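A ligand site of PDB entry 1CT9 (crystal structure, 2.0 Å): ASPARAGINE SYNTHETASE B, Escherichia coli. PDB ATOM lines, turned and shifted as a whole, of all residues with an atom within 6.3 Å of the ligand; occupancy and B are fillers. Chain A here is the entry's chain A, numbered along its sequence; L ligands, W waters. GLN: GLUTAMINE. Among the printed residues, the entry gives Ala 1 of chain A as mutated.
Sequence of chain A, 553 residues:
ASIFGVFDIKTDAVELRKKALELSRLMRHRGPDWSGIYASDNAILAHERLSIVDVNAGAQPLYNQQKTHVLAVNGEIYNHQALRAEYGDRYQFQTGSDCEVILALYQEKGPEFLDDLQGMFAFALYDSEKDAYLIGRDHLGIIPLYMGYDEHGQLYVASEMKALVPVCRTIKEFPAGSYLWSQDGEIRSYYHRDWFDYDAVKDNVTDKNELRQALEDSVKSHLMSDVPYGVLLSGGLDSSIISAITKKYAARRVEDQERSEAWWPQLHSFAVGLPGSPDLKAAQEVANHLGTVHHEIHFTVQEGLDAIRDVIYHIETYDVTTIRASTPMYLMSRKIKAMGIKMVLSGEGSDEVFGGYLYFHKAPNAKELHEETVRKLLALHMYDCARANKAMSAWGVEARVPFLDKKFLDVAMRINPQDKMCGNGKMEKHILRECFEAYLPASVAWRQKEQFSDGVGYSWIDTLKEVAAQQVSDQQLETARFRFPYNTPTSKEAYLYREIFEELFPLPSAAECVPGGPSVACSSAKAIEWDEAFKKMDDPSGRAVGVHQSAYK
The guanidinium group (NH2) of Arg 49 lies within salt-bridge range of an oxygen (O) of the ligand, at 3.0 Å. N of Gly 75 is in hydrogen-bond range of OE1 of the ligand, at 2.5 Å. The side-chain carboxylate (OE1) of Glu 76 is in salt-bridge range of a nitrogen (N) of the ligand, at 3.1 Å. The backbone NH (N) of Val 53 sits at hydrogen-bond distance from an oxygen (OXT) of the ligand (2.8 Å). OD1 of Asp 98 is in salt-bridge range of N of the ligand (2.6 Å). O of Leu 50 lies within hydrogen-bond range of NE2 of the ligand. The side-chain amide nitrogen of Asn 74 sits at hydrogen-bond distance from an oxygen (OE1) of the ligand, at 3.0 Å. A nitrogen (N) of the ligand is in hydrogen-bond range of the backbone carbonyl oxygen of Gly 75, 3.1 Å away. The backbone NH of Ile 52 is in hydrogen-bond range of an oxygen (OXT) of the ligand (2.8 Å).
OE1 of Glu 76 lies close to OE2 of Glu 398 (2.5 Å). The guanidinium group (NE) of Arg 30 sits at hydrogen-bond distance from the backbone carbonyl oxygen (O) of Ala 1 (2.8 Å). OE1 of Glu 76 is in salt-bridge range of NH2 of Arg 400 (3.6 Å). O of Gly 58 lies close to NE of Arg 49. N of Glu 76 lies within hydrogen-bond range of O of Met 120 (2.8 Å). The guanidinium group (NH2) of Arg 30 sits at hydrogen-bond distance from the side-chain amide oxygen (OD1) of Asn 74 (2.8 Å). The backbone NH of Ile 77 lies within hydrogen-bond range of the side-chain carboxylate of Asp 98 (2.8 Å). The backbone carbonyl oxygen of Ala 1 lies close to the side-chain amide nitrogen of Asn 74, 3.1 Å away.
N of Ala 1 lies close to NE2 of the ligand (3.0 Å). Merely in contact with the ligand: Ser 51 (3.9 Å), Cys 99 (3.98 Å) and Glu 398 (3.999 Å). Hydrophobic or aromatic side chains that line the ligand: Ala 1, Leu 50, Ile 52 and Val 53.
Water W2 lies within hydrogen-bond range of the side-chain carboxylate of Glu 398, an oxygen (OE1) of the ligand and the backbone NH of Gly 75. Water W1 lies within hydrogen-bond range of O of Gly 58 (2.5 Å), OG of Ser 97 (2.8 Å), O of the ligand (2.9 Å) and NE2 of Gln 60 (3.1 Å).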
ATOM      1  N   ALA A   1     -22.111   5.387 -24.363  1.00  0.00           N
ATOM      2  CA  ALA A   1     -22.443   6.796 -24.271  1.00  0.00           C
ATOM      3  C   ALA A   1     -23.710   6.965 -23.459  1.00  0.00           C
ATOM      4  O   ALA A   1     -24.397   6.017 -23.050  1.00  0.00           O
ATOM      5  CB  ALA A   1     -22.791   7.292 -25.673  1.00  0.00           C
ATOM      6  N   SER A   2     -24.063   8.214 -23.287  1.00  0.00           N
ATOM      7  CA  SER A   2     -25.287   8.572 -22.631  1.00  0.00           C
ATOM      8  C   SER A   2     -26.041   9.553 -23.520  1.00  0.00           C
ATOM      9  O   SER A   2     -25.395  10.316 -24.265  1.00  0.00           O
ATOM     10  CB  SER A   2     -25.090   9.230 -21.245  1.00  0.00           C
ATOM     11  OG  SER A   2     -24.468  10.501 -21.337  1.00  0.00           O
ATOM     12  N   ARG A  30     -20.412   7.089 -18.857  1.00  0.00           N
ATOM     13  CA  ARG A  30     -20.763   6.279 -19.980  1.00  0.00           C
ATOM     14  C   ARG A  30     -20.180   6.825 -21.291  1.00  0.00           C
ATOM     15  O   ARG A  30     -20.077   6.026 -22.231  1.00  0.00           O
ATOM     16  CB  ARG A  30     -22.250   5.981 -20.191  1.00  0.00           C
ATOM     17  CG  ARG A  30     -23.166   5.951 -19.001  1.00  0.00           C
ATOM     18  CD  ARG A  30     -24.656   5.885 -19.387  1.00  0.00           C
ATOM     19  NE  ARG A  30     -25.029   4.968 -20.482  1.00  0.00           N
ATOM     20  CZ  ARG A  30     -25.267   3.667 -20.307  1.00  0.00           C
ATOM     21  NH1 ARG A  30     -25.164   3.086 -19.129  1.00  0.00           N
ATOM     22  NH2 ARG A  30     -25.634   2.894 -21.325  1.00  0.00           N
ATOM     23  N   HIS A  47     -25.484  14.793 -25.293  1.00  0.00           N
ATOM     24  CA  HIS A  47     -24.881  13.461 -25.478  1.00  0.00           C
ATOM     25  C   HIS A  47     -23.492  13.377 -24.871  1.00  0.00           C
ATOM     26  O   HIS A  47     -22.795  14.376 -24.866  1.00  0.00           O
ATOM     27  CB  HIS A  47     -24.840  13.183 -27.010  1.00  0.00           C
ATOM     28  CG  HIS A  47     -24.407  11.805 -27.417  1.00  0.00           C
ATOM     29  ND1 HIS A  47     -23.045  11.427 -27.430  1.00  0.00           N
ATOM     30  CD2 HIS A  47     -25.155  10.752 -27.853  1.00  0.00           C
ATOM     31  CE1 HIS A  47     -23.027  10.139 -27.843  1.00  0.00           C
ATOM     32  NE2 HIS A  47     -24.286   9.685 -28.091  1.00  0.00           N
ATOM     33  N   GLU A  48     -23.142  12.215 -24.315  1.00  0.00           N
ATOM     34  CA  GLU A  48     -21.806  12.045 -23.780  1.00  0.00           C
ATOM     35  C   GLU A  48     -21.338  10.827 -24.547  1.00  0.00           C
ATOM     36  O   GLU A  48     -22.000   9.755 -24.572  1.00  0.00           O
ATOM     37  CB  GLU A  48     -21.707  11.825 -22.256  1.00  0.00           C
ATOM     38  CG  GLU A  48     -22.465  12.861 -21.377  1.00  0.00           C
ATOM     39  CD  GLU A  48     -21.693  14.135 -21.160  1.00  0.00           C
ATOM     40  OE1 GLU A  48     -22.185  15.248 -20.936  1.00  0.00           O
ATOM     41  OE2 GLU A  48     -20.409  13.930 -21.253  1.00  0.00           O
ATOM     42  N   ARG A  49     -20.244  10.991 -25.276  1.00  0.00           N
ATOM     43  CA  ARG A  49     -19.770   9.909 -26.142  1.00  0.00           C
ATOM     44  C   ARG A  49     -18.631   8.952 -25.694  1.00  0.00           C
ATOM     45  O   ARG A  49     -17.669   9.324 -25.023  1.00  0.00           O
ATOM     46  CB  ARG A  49     -19.350  10.565 -27.455  1.00  0.00           C
ATOM     47  CG  ARG A  49     -19.459   9.636 -28.662  1.00  0.00           C
ATOM     48  CD  ARG A  49     -18.887  10.203 -29.955  1.00  0.00           C
ATOM     49  NE  ARG A  49     -18.717   9.142 -30.934  1.00  0.00           N
ATOM     50  CZ  ARG A  49     -17.879   9.167 -31.973  1.00  0.00           C
ATOM     51  NH1 ARG A  49     -17.119  10.242 -32.232  1.00  0.00           N
ATOM     52  NH2 ARG A  49     -17.841   8.099 -32.759  1.00  0.00           N
ATOM     53  N   LEU A  50     -18.790   7.714 -26.161  1.00  0.00           N
ATOM     54  CA  LEU A  50     -17.856   6.597 -26.109  1.00  0.00           C
ATOM     55  C   LEU A  50     -17.763   6.170 -27.583  1.00  0.00           C
ATOM     56  O   LEU A  50     -18.653   5.476 -28.063  1.00  0.00           O
ATOM     57  CB  LEU A  50     -18.171   5.398 -25.207  1.00  0.00           C
ATOM     58  CG  LEU A  50     -17.122   4.289 -25.334  1.00  0.00           C
ATOM     59  CD1 LEU A  50     -15.916   4.633 -24.467  1.00  0.00           C
ATOM     60  CD2 LEU A  50     -17.642   3.049 -24.679  1.00  0.00           C
ATOM     61  N   SER A  51     -16.701   6.619 -28.279  1.00  0.00           N
ATOM     62  CA  SER A  51     -16.434   6.456 -29.704  1.00  0.00           C
ATOM     63  C   SER A  51     -15.971   5.103 -30.074  1.00  0.00           C
ATOM     64  O   SER A  51     -14.860   4.765 -29.758  1.00  0.00           O
ATOM     65  CB  SER A  51     -15.367   7.464 -30.038  1.00  0.00           C
ATOM     66  OG  SER A  51     -15.822   8.773 -29.733  1.00  0.00           O
ATOM     67  N   ILE A  52     -16.814   4.307 -30.714  1.00  0.00           N
ATOM     68  CA  ILE A  52     -16.404   2.953 -31.042  1.00  0.00           C
ATOM     69  C   ILE A  52     -16.239   2.786 -32.535  1.00  0.00           C
ATOM     70  O   ILE A  52     -15.297   2.196 -33.066  1.00  0.00           O
ATOM     71  CB  ILE A  52     -17.392   1.965 -30.462  1.00  0.00           C
ATOM     72  CG1 ILE A  52     -17.570   2.176 -28.951  1.00  0.00           C
ATOM     73  CG2 ILE A  52     -17.088   0.515 -30.777  1.00  0.00           C
ATOM     74  CD1 ILE A  52     -16.434   1.655 -28.107  1.00  0.00           C
ATOM     75  N   VAL A  53     -17.205   3.376 -33.210  1.00  0.00           N
ATOM     76  CA  VAL A  53     -17.318   3.401 -34.653  1.00  0.00           C
ATOM     77  C   VAL A  53     -17.210   4.823 -35.197  1.00  0.00           C
ATOM     78  O   VAL A  53     -17.922   5.752 -34.809  1.00  0.00           O
ATOM     79  CB  VAL A  53     -18.653   2.774 -35.033  1.00  0.00           C
ATOM     80  CG1 VAL A  53     -18.951   2.894 -36.521  1.00  0.00           C
ATOM     81  CG2 VAL A  53     -18.701   1.327 -34.573  1.00  0.00           C
ATOM     82  N   ASP A  54     -16.280   5.000 -36.132  1.00  0.00           N
ATOM     83  CA  ASP A  54     -16.018   6.273 -36.780  1.00  0.00           C
ATOM     84  C   ASP A  54     -15.720   7.290 -35.736  1.00  0.00           C
ATOM     85  O   ASP A  54     -16.496   8.204 -35.486  1.00  0.00           O
ATOM     86  CB  ASP A  54     -17.149   6.714 -37.713  1.00  0.00           C
ATOM     87  CG  ASP A  54     -17.009   8.099 -38.289  1.00  0.00           C
ATOM     88  OD1 ASP A  54     -17.986   8.744 -38.692  1.00  0.00           O
ATOM     89  OD2 ASP A  54     -15.745   8.516 -38.336  1.00  0.00           O
ATOM     90  N   GLY A  58     -17.793  10.607 -35.993  1.00  0.00           N
ATOM     91  CA  GLY A  58     -18.990   9.993 -35.422  1.00  0.00           C
ATOM     92  C   GLY A  58     -19.663  10.783 -34.276  1.00  0.00           C
ATOM     93  O   GLY A  58     -20.530  10.269 -33.584  1.00  0.00           O
ATOM     94  N   ALA A  59     -19.275  12.042 -34.079  1.00  0.00           N
ATOM     95  CA  ALA A  59     -19.811  12.905 -33.044  1.00  0.00           C
ATOM     96  C   ALA A  59     -21.336  13.060 -32.984  1.00  0.00           C
ATOM     97  O   ALA A  59     -22.051  13.062 -33.996  1.00  0.00           O
ATOM     98  CB  ALA A  59     -19.204  14.288 -33.235  1.00  0.00           C
ATOM     99  N   GLN A  60     -21.853  13.222 -31.770  1.00  0.00           N
ATOM    100  CA  GLN A  60     -23.269  13.436 -31.603  1.00  0.00           C
ATOM    101  C   GLN A  60     -23.547  14.595 -30.656  1.00  0.00           C
ATOM    102  O   GLN A  60     -22.715  14.997 -29.867  1.00  0.00           O
ATOM    103  CB  GLN A  60     -23.982  12.237 -31.033  1.00  0.00           C
ATOM    104  CG  GLN A  60     -23.408  10.932 -31.559  1.00  0.00           C
ATOM    105  CD  GLN A  60     -24.526   9.953 -31.378  1.00  0.00           C
ATOM    106  OE1 GLN A  60     -25.621  10.435 -31.063  1.00  0.00           O
ATOM    107  NE2 GLN A  60     -24.312   8.654 -31.549  1.00  0.00           N
ATOM    108  N   VAL A  73     -27.977   9.153 -29.818  1.00  0.00           N
ATOM    109  CA  VAL A  73     -28.074   7.721 -29.610  1.00  0.00           C
ATOM    110  C   VAL A  73     -26.945   7.096 -28.775  1.00  0.00           C
ATOM    111  O   VAL A  73     -25.782   7.450 -28.871  1.00  0.00           O
ATOM    112  CB  VAL A  73     -28.003   7.008 -30.966  1.00  0.00           C
ATOM    113  CG1 VAL A  73     -28.145   5.484 -30.914  1.00  0.00           C
ATOM    114  CG2 VAL A  73     -28.865   7.666 -32.041  1.00  0.00           C
ATOM    115  N   ASN A  74     -27.362   6.100 -28.006  1.00  0.00           N
ATOM    116  CA  ASN A  74     -26.518   5.245 -27.202  1.00  0.00           C
ATOM    117  C   ASN A  74     -26.743   3.849 -27.784  1.00  0.00           C
ATOM    118  O   ASN A  74     -27.779   3.197 -27.603  1.00  0.00           O
ATOM    119  CB  ASN A  74     -26.783   5.344 -25.681  1.00  0.00           C
ATOM    120  CG  ASN A  74     -26.076   4.295 -24.805  1.00  0.00           C
ATOM    121  OD1 ASN A  74     -26.624   3.831 -23.792  1.00  0.00           O
ATOM    122  ND2 ASN A  74     -24.868   3.874 -25.186  1.00  0.00           N
ATOM    123  N   GLY A  75     -25.803   3.374 -28.606  1.00  0.00           N
ATOM    124  CA  GLY A  75     -26.054   2.069 -29.172  1.00  0.00           C
ATOM    125  C   GLY A  75     -25.107   1.702 -30.315  1.00  0.00           C
ATOM    126  O   GLY A  75     -24.149   2.388 -30.583  1.00  0.00           O
ATOM    127  N   GLU A  76     -25.397   0.537 -30.924  1.00  0.00           N
ATOM    128  CA  GLU A  76     -24.644   0.016 -32.041  1.00  0.00           C
ATOM    129  C   GLU A  76     -25.661  -0.534 -33.009  1.00  0.00           C
ATOM    130  O   GLU A  76     -26.487  -1.405 -32.636  1.00  0.00           O
ATOM    131  CB  GLU A  76     -23.739  -1.149 -31.610  1.00  0.00           C
ATOM    132  CG  GLU A  76     -22.660  -0.683 -30.651  1.00  0.00           C
ATOM    133  CD  GLU A  76     -21.702   0.316 -31.233  1.00  0.00           C
ATOM    134  OE1 GLU A  76     -20.960   0.998 -30.556  1.00  0.00           O
ATOM    135  OE2 GLU A  76     -21.687   0.334 -32.541  1.00  0.00           O
ATOM    136  N   ILE A  77     -25.644  -0.035 -34.248  1.00  0.00           N
ATOM    137  CA  ILE A  77     -26.599  -0.596 -35.211  1.00  0.00           C
ATOM    138  C   ILE A  77     -25.843  -1.533 -36.151  1.00  0.00           C
ATOM    139  O   ILE A  77     -25.189  -1.060 -37.072  1.00  0.00           O
ATOM    140  CB  ILE A  77     -27.493   0.428 -35.919  1.00  0.00           C
ATOM    141  CG1 ILE A  77     -28.371   1.099 -34.850  1.00  0.00           C
ATOM    142  CG2 ILE A  77     -28.412  -0.328 -36.887  1.00  0.00           C
ATOM    143  CD1 ILE A  77     -27.858   2.505 -34.632  1.00  0.00           C
ATOM    144  N   SER A  97     -20.810   7.145 -38.783  1.00  0.00           N
ATOM    145  CA  SER A  97     -21.471   6.561 -37.629  1.00  0.00           C
ATOM    146  C   SER A  97     -22.550   5.537 -37.970  1.00  0.00           C
ATOM    147  O   SER A  97     -23.461   5.778 -38.772  1.00  0.00           O
ATOM    148  CB  SER A  97     -21.965   7.631 -36.674  1.00  0.00           C
ATOM    149  OG  SER A  97     -22.860   7.058 -35.756  1.00  0.00           O
ATOM    150  N   ASP A  98     -22.453   4.367 -37.321  1.00  0.00           N
ATOM    151  CA  ASP A  98     -23.442   3.336 -37.468  1.00  0.00           C
ATOM    152  C   ASP A  98     -24.851   3.881 -37.094  1.00  0.00           C
ATOM    153  O   ASP A  98     -25.870   3.417 -37.587  1.00  0.00           O
ATOM    154  CB  ASP A  98     -23.091   2.149 -36.584  1.00  0.00           C
ATOM    155  CG  ASP A  98     -22.969   2.569 -35.125  1.00  0.00           C
ATOM    156  OD1 ASP A  98     -22.057   3.208 -34.725  1.00  0.00           O
ATOM    157  OD2 ASP A  98     -23.986   2.251 -34.347  1.00  0.00           O
ATOM    158  N   CYS A  99     -24.890   4.862 -36.203  1.00  0.00           N
ATOM    159  CA  CYS A  99     -26.108   5.470 -35.718  1.00  0.00           C
ATOM    160  C   CYS A  99     -26.875   6.455 -36.656  1.00  0.00           C
ATOM    161  O   CYS A  99     -28.093   6.698 -36.597  1.00  0.00           O
ATOM    162  CB  CYS A  99     -25.702   6.090 -34.340  1.00  0.00           C
ATOM    163  SG  CYS A  99     -25.589   4.848 -33.006  1.00  0.00           S
ATOM    164  N   MET A 120     -28.424  -2.715 -30.755  1.00  0.00           N
ATOM    165  CA  MET A 120     -28.875  -2.350 -29.435  1.00  0.00           C
ATOM    166  C   MET A 120     -28.873  -0.835 -29.418  1.00  0.00           C
ATOM    167  O   MET A 120     -27.964  -0.174 -29.952  1.00  0.00           O
ATOM    168  CB  MET A 120     -28.012  -2.985 -28.314  1.00  0.00           C
ATOM    169  CG  MET A 120     -26.506  -2.741 -28.503  1.00  0.00           C
ATOM    170  SD  MET A 120     -25.486  -3.233 -27.085  1.00  0.00           S
ATOM    171  CE  MET A 120     -23.978  -2.286 -27.389  1.00  0.00           C
ATOM    172  N   ILE A 143     -29.916  -1.796 -24.254  1.00  0.00           N
ATOM    173  CA  ILE A 143     -29.385  -0.539 -23.817  1.00  0.00           C
ATOM    174  C   ILE A 143     -30.450   0.080 -22.911  1.00  0.00           C
ATOM    175  O   ILE A 143     -31.665  -0.028 -23.188  1.00  0.00           O
ATOM    176  CB  ILE A 143     -29.175   0.329 -25.025  1.00  0.00           C
ATOM    177  CG1 ILE A 143     -27.958  -0.173 -25.758  1.00  0.00           C
ATOM    178  CG2 ILE A 143     -29.014   1.802 -24.655  1.00  0.00           C
ATOM    179  CD1 ILE A 143     -26.644   0.338 -25.196  1.00  0.00           C
ATOM    180  N   MET A 224     -18.163  -5.400 -35.176  1.00  0.00           N
ATOM    181  CA  MET A 224     -18.112  -4.104 -35.796  1.00  0.00           C
ATOM    182  C   MET A 224     -17.431  -3.052 -34.930  1.00  0.00           C
ATOM    183  O   MET A 224     -17.929  -2.702 -33.872  1.00  0.00           O
ATOM    184  CB  MET A 224     -19.522  -3.727 -36.222  1.00  0.00           C
ATOM    185  CG  MET A 224     -19.650  -2.249 -36.485  1.00  0.00           C
ATOM    186  SD  MET A 224     -21.333  -1.803 -37.051  1.00  0.00           S
ATOM    187  CE  MET A 224     -21.865  -0.831 -35.613  1.00  0.00           C
ATOM    188  N   GLU A 398     -18.168  -0.569 -23.452  1.00  0.00           N
ATOM    189  CA  GLU A 398     -19.338  -1.069 -24.147  1.00  0.00           C
ATOM    190  C   GLU A 398     -19.419  -2.582 -24.198  1.00  0.00           C
ATOM    191  O   GLU A 398     -18.453  -3.211 -24.578  1.00  0.00           O
ATOM    192  CB  GLU A 398     -19.410  -0.505 -25.553  1.00  0.00           C
ATOM    193  CG  GLU A 398     -20.558  -1.105 -26.374  1.00  0.00           C
ATOM    194  CD  GLU A 398     -20.467  -0.727 -27.827  1.00  0.00           C
ATOM    195  OE1 GLU A 398     -19.818  -1.334 -28.622  1.00  0.00           O
ATOM    196  OE2 GLU A 398     -21.110   0.354 -28.134  1.00  0.00           O
ATOM    197  N   ARG A 400     -21.270  -6.103 -25.612  1.00  0.00           N
ATOM    198  CA  ARG A 400     -22.073  -6.617 -26.691  1.00  0.00           C
ATOM    199  C   ARG A 400     -22.502  -7.976 -26.287  1.00  0.00           C
ATOM    200  O   ARG A 400     -21.747  -8.631 -25.567  1.00  0.00           O
ATOM    201  CB  ARG A 400     -21.331  -6.599 -28.003  1.00  0.00           C
ATOM    202  CG  ARG A 400     -20.733  -5.212 -28.253  1.00  0.00           C
ATOM    203  CD  ARG A 400     -20.505  -4.973 -29.729  1.00  0.00           C
ATOM    204  NE  ARG A 400     -20.099  -3.591 -29.999  1.00  0.00           N
ATOM    205  CZ  ARG A 400     -19.561  -3.222 -31.165  1.00  0.00           C
ATOM    206  NH1 ARG A 400     -19.417  -4.106 -32.124  1.00  0.00           N
ATOM    207  NH2 ARG A 400     -19.167  -1.963 -31.393  1.00  0.00           N
HETATM  208  N   GLN L   1     -21.721   3.496 -32.200  1.00  0.00           N
HETATM  209  CA  GLN L   1     -21.767   4.788 -31.910  1.00  0.00           C
HETATM  210  C   GLN L   1     -20.332   5.247 -31.824  1.00  0.00           C
HETATM  211  O   GLN L   1     -20.110   6.486 -31.723  1.00  0.00           O
HETATM  212  CB  GLN L   1     -22.393   5.014 -30.511  1.00  0.00           C
HETATM  213  CG  GLN L   1     -21.741   4.062 -29.491  1.00  0.00           C
HETATM  214  CD  GLN L   1     -22.297   4.196 -28.076  1.00  0.00           C
HETATM  215  OE1 GLN L   1     -23.468   3.916 -27.804  1.00  0.00           O
HETATM  216  NE2 GLN L   1     -21.446   4.608 -27.157  1.00  0.00           N
HETATM  217  OXT GLN L   1     -19.374   4.389 -31.813  1.00  0.00           O
HETATM  218  O   HOH W   1     -21.826   8.143 -33.347  1.00  0.00           O
HETATM  219  O   HOH W   2     -23.506   1.161 -27.289  1.00  0.00           O
